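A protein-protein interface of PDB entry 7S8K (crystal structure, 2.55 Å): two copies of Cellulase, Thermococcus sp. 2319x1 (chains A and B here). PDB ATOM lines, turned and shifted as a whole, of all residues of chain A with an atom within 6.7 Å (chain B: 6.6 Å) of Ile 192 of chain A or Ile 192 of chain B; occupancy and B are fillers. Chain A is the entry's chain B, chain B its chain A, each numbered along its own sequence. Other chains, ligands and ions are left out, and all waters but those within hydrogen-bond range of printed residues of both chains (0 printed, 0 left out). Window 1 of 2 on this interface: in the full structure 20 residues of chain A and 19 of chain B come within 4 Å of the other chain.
Among the printed residues, pairs that only touch across the chains: Asn 70 of chain A with Trp 194 of chain B (3.9 Å), Asn 70 of chain A with Glu 195 of chain B (3.8 Å), Asn 191 of chain A with Ile 192 of chain B (3.9 Å), Ile 192 of chain A with Gly 193 of chain B (3.9 Å), Gly 193 of chain A with Ile 192 of chain B (3.8 Å), Trp 194 of chain A with Asn 70 of chain B (3.9 Å) and Glu 195 of chain A with Asn 70 of chain B (3.7 Å).
Asn 70 of chain A touches Asn 191 of chain B, and with the chains exchanged Asn 191 of chain A touches Asn 70 of chain B. Asn 70 of chain A touches Glu 195 of chain B, and with the chains exchanged Glu 195 of chain A touches Asn 70 of chain B. Asn 191 of chain A touches Ile 192 of chain B, but with the chains exchanged Ile 192 of chain A does not touch Asn 191 of chain B (4.4 Å). Ile 192 of chain B touches its own counterpart, Ile 192 of chain A. Positions printed for both chains: 70, 150, 163, 164, 190, 191, 192, 193, 194, 195 and 196.
OD1 of Asn 70 of chain B lies within hydrogen-bond range of N of Gly 72 of chain B, 3.1 Å away. NE1 of Trp 194 of chain B sits at hydrogen-bond distance from OE1 of Glu 150 of chain B (2.8 Å). The backbone NH (N) of Glu 150 of chain B lies within hydrogen-bond range of the backbone carbonyl oxygen (O) of Glu 195 of chain B. The side-chain carboxylate of Glu 150 of chain A sits at hydrogen-bond distance from the indole nitrogen of Trp 194 of chain A. N of Glu 150 of chain A is in hydrogen-bond range of O of Glu 195 of chain A.
Of chain A, only Asn 191, Ile 192 and Gly 193 come within 4 Å of Ile 192 of chain B. Of the printed residues of chain A, Asn 70 of chain B touches Asn 191, Trp 194 and Glu 195. Of the printed residues of chain B, Asn 191 of chain A touches Asn 70 (2.9 Å), Gly 72 (3.2 Å) and Ile 192 (3.9 Å). Printed residues of chain B within 4 Å of Glu 195 of chain A: Asn 70. Ala 163 of chain A touches none of the printed residues of chain B. Tyr 196 of chain B touches none of the printed residues of chain A.
The side-chain amide nitrogen of Asn 191 of chain A sits at hydrogen-bond distance from the side-chain amide oxygen of Asn 70 of chain B, at 2.9 Å. The side-chain amide oxygen (OD1) of Asn 191 of chain A sits close to the backbone carbonyl oxygen (O) of Gly 72 of chain B, 3.4 Å away. The side-chain amide oxygen of Asn 191 of chain B sits at hydrogen-bond distance from the side-chain amide nitrogen of Asn 70 of chain A, 2.9 Å away. The backbone carbonyl oxygen of Ile 192 of chain A lies close to the backbone carbonyl oxygen of Ile 192 of chain B, 2.7 Å away.
Printed residues of chain A that touch a printed residue of chain B: Asn 70, Asn 191, Ile 192, Gly 193, Trp 194 and Glu 195. Hydrophobic or aromatic side chains of chain A within 4 Å of the printed part of chain B: Ile 192. Of the 12 printed residues of chain B, 7 touch a printed residue of chain A. Hydrophobic or aromatic side chains of chain B that line the printed part of chain A: Ile 192. Among the printed residues, 11 pairs touch across the chains. Among the printed residues, no Asp or Glu carboxylate lies within 4 Å of a Lys or Arg side-chain nitrogen of the other chain.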
ATOM      1  N   ASN A  70      15.200  18.213 -18.931  1.00  0.00           N
ATOM      2  CA  ASN A  70      15.765  17.307 -19.926  1.00  0.00           C
ATOM      3  C   ASN A  70      14.925  17.456 -21.189  1.00  0.00           C
ATOM      4  O   ASN A  70      13.794  16.963 -21.250  1.00  0.00           O
ATOM      5  CB  ASN A  70      15.776  15.867 -19.422  1.00  0.00           C
ATOM      6  CG  ASN A  70      16.593  14.946 -20.304  1.00  0.00           C
ATOM      7  OD1 ASN A  70      17.099  15.357 -21.349  1.00  0.00           O
ATOM      8  ND2 ASN A  70      16.725  13.692 -19.891  1.00  0.00           N
ATOM      9  N   GLU A 150       6.892   0.120 -15.947  1.00  0.00           N
ATOM     10  CA  GLU A 150       5.979   1.256 -15.943  1.00  0.00           C
ATOM     11  C   GLU A 150       4.854   0.958 -16.923  1.00  0.00           C
ATOM     12  O   GLU A 150       5.108   0.737 -18.114  1.00  0.00           O
ATOM     13  CB  GLU A 150       6.688   2.555 -16.331  1.00  0.00           C
ATOM     14  CG  GLU A 150       5.735   3.735 -16.484  1.00  0.00           C
ATOM     15  CD  GLU A 150       6.407   4.977 -17.038  1.00  0.00           C
ATOM     16  OE1 GLU A 150       7.584   4.891 -17.443  1.00  0.00           O
ATOM     17  OE2 GLU A 150       5.752   6.042 -17.064  1.00  0.00           O
ATOM     18  N   ALA A 163       6.465   6.293 -25.805  1.00  0.00           N
ATOM     19  CA  ALA A 163       7.850   5.943 -26.068  1.00  0.00           C
ATOM     20  C   ALA A 163       7.941   4.550 -26.683  1.00  0.00           C
ATOM     21  O   ALA A 163       7.055   3.707 -26.522  1.00  0.00           O
ATOM     22  CB  ALA A 163       8.677   6.008 -24.783  1.00  0.00           C
ATOM     23  N   GLY A 164       9.033   4.315 -27.403  1.00  0.00           N
ATOM     24  CA  GLY A 164       9.272   2.997 -27.956  1.00  0.00           C
ATOM     25  C   GLY A 164       8.464   2.728 -29.214  1.00  0.00           C
ATOM     26  O   GLY A 164       8.178   3.627 -30.007  1.00  0.00           O
ATOM     27  N   ALA A 190       8.624   0.266 -24.835  1.00  0.00           N
ATOM     28  CA  ALA A 190       9.905   0.950 -24.779  1.00  0.00           C
ATOM     29  C   ALA A 190      10.731   0.353 -23.653  1.00  0.00           C
ATOM     30  O   ALA A 190      10.189  -0.156 -22.667  1.00  0.00           O
ATOM     31  CB  ALA A 190       9.736   2.456 -24.547  1.00  0.00           C
ATOM     32  N   ASN A 191      12.050   0.414 -23.802  1.00  0.00           N
ATOM     33  CA  ASN A 191      12.959   0.032 -22.729  1.00  0.00           C
ATOM     34  C   ASN A 191      13.863   1.219 -22.432  1.00  0.00           C
ATOM     35  O   ASN A 191      14.767   1.536 -23.214  1.00  0.00           O
ATOM     36  CB  ASN A 191      13.759  -1.217 -23.083  1.00  0.00           C
ATOM     37  CG  ASN A 191      14.149  -2.008 -21.853  1.00  0.00           C
ATOM     38  OD1 ASN A 191      15.101  -1.663 -21.150  1.00  0.00           O
ATOM     39  ND2 ASN A 191      13.367  -3.040 -21.549  1.00  0.00           N
ATOM     40  N   ILE A 192      13.610   1.866 -21.298  1.00  0.00           N
ATOM     41  CA  ILE A 192      14.215   3.143 -20.945  1.00  0.00           C
ATOM     42  C   ILE A 192      14.866   3.063 -19.569  1.00  0.00           C
ATOM     43  O   ILE A 192      14.563   3.862 -18.675  1.00  0.00           O
ATOM     44  CB  ILE A 192      13.153   4.258 -21.009  1.00  0.00           C
ATOM     45  CG1 ILE A 192      11.974   3.925 -20.090  1.00  0.00           C
ATOM     46  CG2 ILE A 192      12.668   4.453 -22.429  1.00  0.00           C
ATOM     47  CD1 ILE A 192      11.018   5.068 -19.886  1.00  0.00           C
ATOM     48  N   GLY A 193      15.778   2.113 -19.383  1.00  0.00           N
ATOM     49  CA  GLY A 193      16.257   1.809 -18.054  1.00  0.00           C
ATOM     50  C   GLY A 193      15.260   1.073 -17.190  1.00  0.00           C
ATOM     51  O   GLY A 193      15.599   0.703 -16.060  1.00  0.00           O
ATOM     52  N   TRP A 194      14.034   0.895 -17.668  1.00  0.00           N
ATOM     53  CA  TRP A 194      13.057  -0.043 -17.134  1.00  0.00           C
ATOM     54  C   TRP A 194      12.102  -0.342 -18.278  1.00  0.00           C
ATOM     55  O   TRP A 194      12.126   0.330 -19.312  1.00  0.00           O
ATOM     56  CB  TRP A 194      12.321   0.517 -15.909  1.00  0.00           C
ATOM     57  CG  TRP A 194      11.634   1.827 -16.151  1.00  0.00           C
ATOM     58  CD1 TRP A 194      10.422   2.019 -16.749  1.00  0.00           C
ATOM     59  CD2 TRP A 194      12.112   3.129 -15.789  1.00  0.00           C
ATOM     60  NE1 TRP A 194      10.121   3.358 -16.790  1.00  0.00           N
ATOM     61  CE2 TRP A 194      11.141   4.061 -16.206  1.00  0.00           C
ATOM     62  CE3 TRP A 194      13.268   3.597 -15.156  1.00  0.00           C
ATOM     63  CZ2 TRP A 194      11.291   5.432 -16.011  1.00  0.00           C
ATOM     64  CZ3 TRP A 194      13.415   4.960 -14.963  1.00  0.00           C
ATOM     65  CH2 TRP A 194      12.431   5.861 -15.390  1.00  0.00           C
ATOM     66  N   GLU A 195      11.264  -1.358 -18.104  1.00  0.00           N
ATOM     67  CA  GLU A 195      10.317  -1.684 -19.159  1.00  0.00           C
ATOM     68  C   GLU A 195       9.146  -0.710 -19.129  1.00  0.00           C
ATOM     69  O   GLU A 195       8.538  -0.480 -18.079  1.00  0.00           O
ATOM     70  CB  GLU A 195       9.817  -3.122 -19.047  1.00  0.00           C
ATOM     71  CG  GLU A 195       9.151  -3.590 -20.333  1.00  0.00           C
ATOM     72  CD  GLU A 195       8.673  -5.018 -20.265  1.00  0.00           C
ATOM     73  OE1 GLU A 195       7.709  -5.291 -19.523  1.00  0.00           O
ATOM     74  OE2 GLU A 195       9.260  -5.867 -20.967  1.00  0.00           O
ATOM     75  N   TYR A 196       8.843  -0.141 -20.291  1.00  0.00           N
ATOM     76  CA  TYR A 196       7.780   0.841 -20.471  1.00  0.00           C
ATOM     77  C   TYR A 196       6.719   0.226 -21.374  1.00  0.00           C
ATOM     78  O   TYR A 196       7.010  -0.139 -22.519  1.00  0.00           O
ATOM     79  CB  TYR A 196       8.355   2.129 -21.068  1.00  0.00           C
ATOM     80  CG  TYR A 196       7.365   3.169 -21.563  1.00  0.00           C
ATOM     81  CD1 TYR A 196       6.753   3.048 -22.808  1.00  0.00           C
ATOM     82  CD2 TYR A 196       7.086   4.300 -20.807  1.00  0.00           C
ATOM     83  CE1 TYR A 196       5.867   4.008 -23.269  1.00  0.00           C
ATOM     84  CE2 TYR A 196       6.203   5.265 -21.261  1.00  0.00           C
ATOM     85  CZ  TYR A 196       5.597   5.114 -22.492  1.00  0.00           C
ATOM     86  OH  TYR A 196       4.720   6.074 -22.944  1.00  0.00           O
ATOM     87  N   ASN B  70      15.898  -8.201 -17.550  1.00  0.00           N
ATOM     88  CA  ASN B  70      15.121  -7.351 -18.449  1.00  0.00           C
ATOM     89  C   ASN B  70      15.674  -7.598 -19.848  1.00  0.00           C
ATOM     90  O   ASN B  70      16.749  -7.097 -20.194  1.00  0.00           O
ATOM     91  CB  ASN B  70      15.216  -5.878 -18.056  1.00  0.00           C
ATOM     92  CG  ASN B  70      14.266  -4.995 -18.854  1.00  0.00           C
ATOM     93  OD1 ASN B  70      13.752  -5.396 -19.899  1.00  0.00           O
ATOM     94  ND2 ASN B  70      14.032  -3.785 -18.360  1.00  0.00           N
ATOM     95  N   GLY B  72      14.739  -6.445 -22.619  1.00  0.00           N
ATOM     96  CA  GLY B  72      14.847  -5.206 -23.358  1.00  0.00           C
ATOM     97  C   GLY B  72      16.071  -4.383 -23.032  1.00  0.00           C
ATOM     98  O   GLY B  72      16.384  -3.454 -23.782  1.00  0.00           O
ATOM     99  N   GLU B 150      24.153   9.843 -18.269  1.00  0.00           N
ATOM    100  CA  GLU B 150      25.052   8.700 -18.360  1.00  0.00           C
ATOM    101  C   GLU B 150      25.977   8.928 -19.546  1.00  0.00           C
ATOM    102  O   GLU B 150      25.516   8.985 -20.692  1.00  0.00           O
ATOM    103  CB  GLU B 150      24.281   7.392 -18.526  1.00  0.00           C
ATOM    104  CG  GLU B 150      25.177   6.199 -18.815  1.00  0.00           C
ATOM    105  CD  GLU B 150      24.420   4.889 -18.898  1.00  0.00           C
ATOM    106  OE1 GLU B 150      23.173   4.915 -18.976  1.00  0.00           O
ATOM    107  OE2 GLU B 150      25.077   3.827 -18.890  1.00  0.00           O
ATOM    108  N   ALA B 163      22.907   2.715 -27.317  1.00  0.00           N
ATOM    109  CA  ALA B 163      21.474   2.946 -27.242  1.00  0.00           C
ATOM    110  C   ALA B 163      21.096   4.236 -27.967  1.00  0.00           C
ATOM    111  O   ALA B 163      21.920   5.128 -28.182  1.00  0.00           O
ATOM    112  CB  ALA B 163      21.017   3.007 -25.784  1.00  0.00           C
ATOM    113  N   GLY B 164      19.829   4.323 -28.350  1.00  0.00           N
ATOM    114  CA  GLY B 164      19.343   5.522 -29.013  1.00  0.00           C
ATOM    115  C   GLY B 164      19.758   5.559 -30.465  1.00  0.00           C
ATOM    116  O   GLY B 164      19.590   4.581 -31.197  1.00  0.00           O
ATOM    117  N   ALA B 190      20.692   8.733 -26.395  1.00  0.00           N
ATOM    118  CA  ALA B 190      19.451   8.084 -26.003  1.00  0.00           C
ATOM    119  C   ALA B 190      18.901   8.783 -24.771  1.00  0.00           C
ATOM    120  O   ALA B 190      19.664   9.226 -23.906  1.00  0.00           O
ATOM    121  CB  ALA B 190      19.664   6.596 -25.707  1.00  0.00           C
ATOM    122  N   ASN B 191      17.581   8.887 -24.688  1.00  0.00           N
ATOM    123  CA  ASN B 191      16.929   9.456 -23.510  1.00  0.00           C
ATOM    124  C   ASN B 191      16.072   8.356 -22.892  1.00  0.00           C
ATOM    125  O   ASN B 191      14.926   8.138 -23.301  1.00  0.00           O
ATOM    126  CB  ASN B 191      16.116  10.693 -23.864  1.00  0.00           C
ATOM    127  CG  ASN B 191      16.243  11.779 -22.816  1.00  0.00           C
ATOM    128  OD1 ASN B 191      15.580  11.745 -21.780  1.00  0.00           O
ATOM    129  ND2 ASN B 191      17.132  12.732 -23.066  1.00  0.00           N
ATOM    130  N   ILE B 192      16.638   7.673 -21.901  1.00  0.00           N
ATOM    131  CA  ILE B 192      16.052   6.460 -21.347  1.00  0.00           C
ATOM    132  C   ILE B 192      15.823   6.621 -19.849  1.00  0.00           C
ATOM    133  O   ILE B 192      16.319   5.831 -19.041  1.00  0.00           O
ATOM    134  CB  ILE B 192      16.945   5.248 -21.690  1.00  0.00           C
ATOM    135  CG1 ILE B 192      18.420   5.494 -21.341  1.00  0.00           C
ATOM    136  CG2 ILE B 192      16.814   4.888 -23.157  1.00  0.00           C
ATOM    137  CD1 ILE B 192      18.901   4.862 -20.068  1.00  0.00           C
ATOM    138  N   GLY B 193      15.047   7.633 -19.468  1.00  0.00           N
ATOM    139  CA  GLY B 193      14.866   7.956 -18.075  1.00  0.00           C
ATOM    140  C   GLY B 193      15.948   8.835 -17.494  1.00  0.00           C
ATOM    141  O   GLY B 193      15.739   9.427 -16.430  1.00  0.00           O
ATOM    142  N   TRP B 194      17.110   8.894 -18.134  1.00  0.00           N
ATOM    143  CA  TRP B 194      18.081   9.963 -17.981  1.00  0.00           C
ATOM    144  C   TRP B 194      18.610  10.266 -19.374  1.00  0.00           C
ATOM    145  O   TRP B 194      18.148   9.693 -20.365  1.00  0.00           O
ATOM    146  CB  TRP B 194      19.214   9.586 -17.018  1.00  0.00           C
ATOM    147  CG  TRP B 194      19.783   8.209 -17.229  1.00  0.00           C
ATOM    148  CD1 TRP B 194      20.848   7.870 -18.014  1.00  0.00           C
ATOM    149  CD2 TRP B 194      19.326   6.990 -16.628  1.00  0.00           C
ATOM    150  NE1 TRP B 194      21.076   6.516 -17.948  1.00  0.00           N
ATOM    151  CE2 TRP B 194      20.159   5.953 -17.100  1.00  0.00           C
ATOM    152  CE3 TRP B 194      18.293   6.674 -15.739  1.00  0.00           C
ATOM    153  CZ2 TRP B 194      19.988   4.624 -16.717  1.00  0.00           C
ATOM    154  CZ3 TRP B 194      18.126   5.354 -15.359  1.00  0.00           C
ATOM    155  CH2 TRP B 194      18.968   4.346 -15.849  1.00  0.00           C
ATOM    156  N   GLU B 195      19.586  11.161 -19.470  1.00  0.00           N
ATOM    157  CA  GLU B 195      20.245  11.387 -20.747  1.00  0.00           C
ATOM    158  C   GLU B 195      21.411  10.420 -20.881  1.00  0.00           C
ATOM    159  O   GLU B 195      22.230  10.290 -19.966  1.00  0.00           O
ATOM    160  CB  GLU B 195      20.727  12.830 -20.893  1.00  0.00           C
ATOM    161  CG  GLU B 195      20.925  13.229 -22.352  1.00  0.00           C
ATOM    162  CD  GLU B 195      21.575  14.588 -22.518  1.00  0.00           C
ATOM    163  OE1 GLU B 195      22.646  14.812 -21.915  1.00  0.00           O
ATOM    164  OE2 GLU B 195      21.020  15.429 -23.257  1.00  0.00           O
ATOM    165  N   TYR B 196      21.473   9.734 -22.017  1.00  0.00           N
ATOM    166  CA  TYR B 196      22.490   8.724 -22.289  1.00  0.00           C
ATOM    167  C   TYR B 196      23.308   9.203 -23.479  1.00  0.00           C
ATOM    168  O   TYR B 196      22.792   9.288 -24.599  1.00  0.00           O
ATOM    169  CB  TYR B 196      21.830   7.367 -22.550  1.00  0.00           C
ATOM    170  CG  TYR B 196      22.702   6.280 -23.149  1.00  0.00           C
ATOM    171  CD1 TYR B 196      22.980   6.243 -24.513  1.00  0.00           C
ATOM    172  CD2 TYR B 196      23.206   5.259 -22.354  1.00  0.00           C
ATOM    173  CE1 TYR B 196      23.758   5.241 -25.058  1.00  0.00           C
ATOM    174  CE2 TYR B 196      23.983   4.251 -22.892  1.00  0.00           C
ATOM    175  CZ  TYR B 196      24.255   4.247 -24.244  1.00  0.00           C
ATOM    176  OH  TYR B 196      25.025   3.244 -24.785  1.00  0.00           O
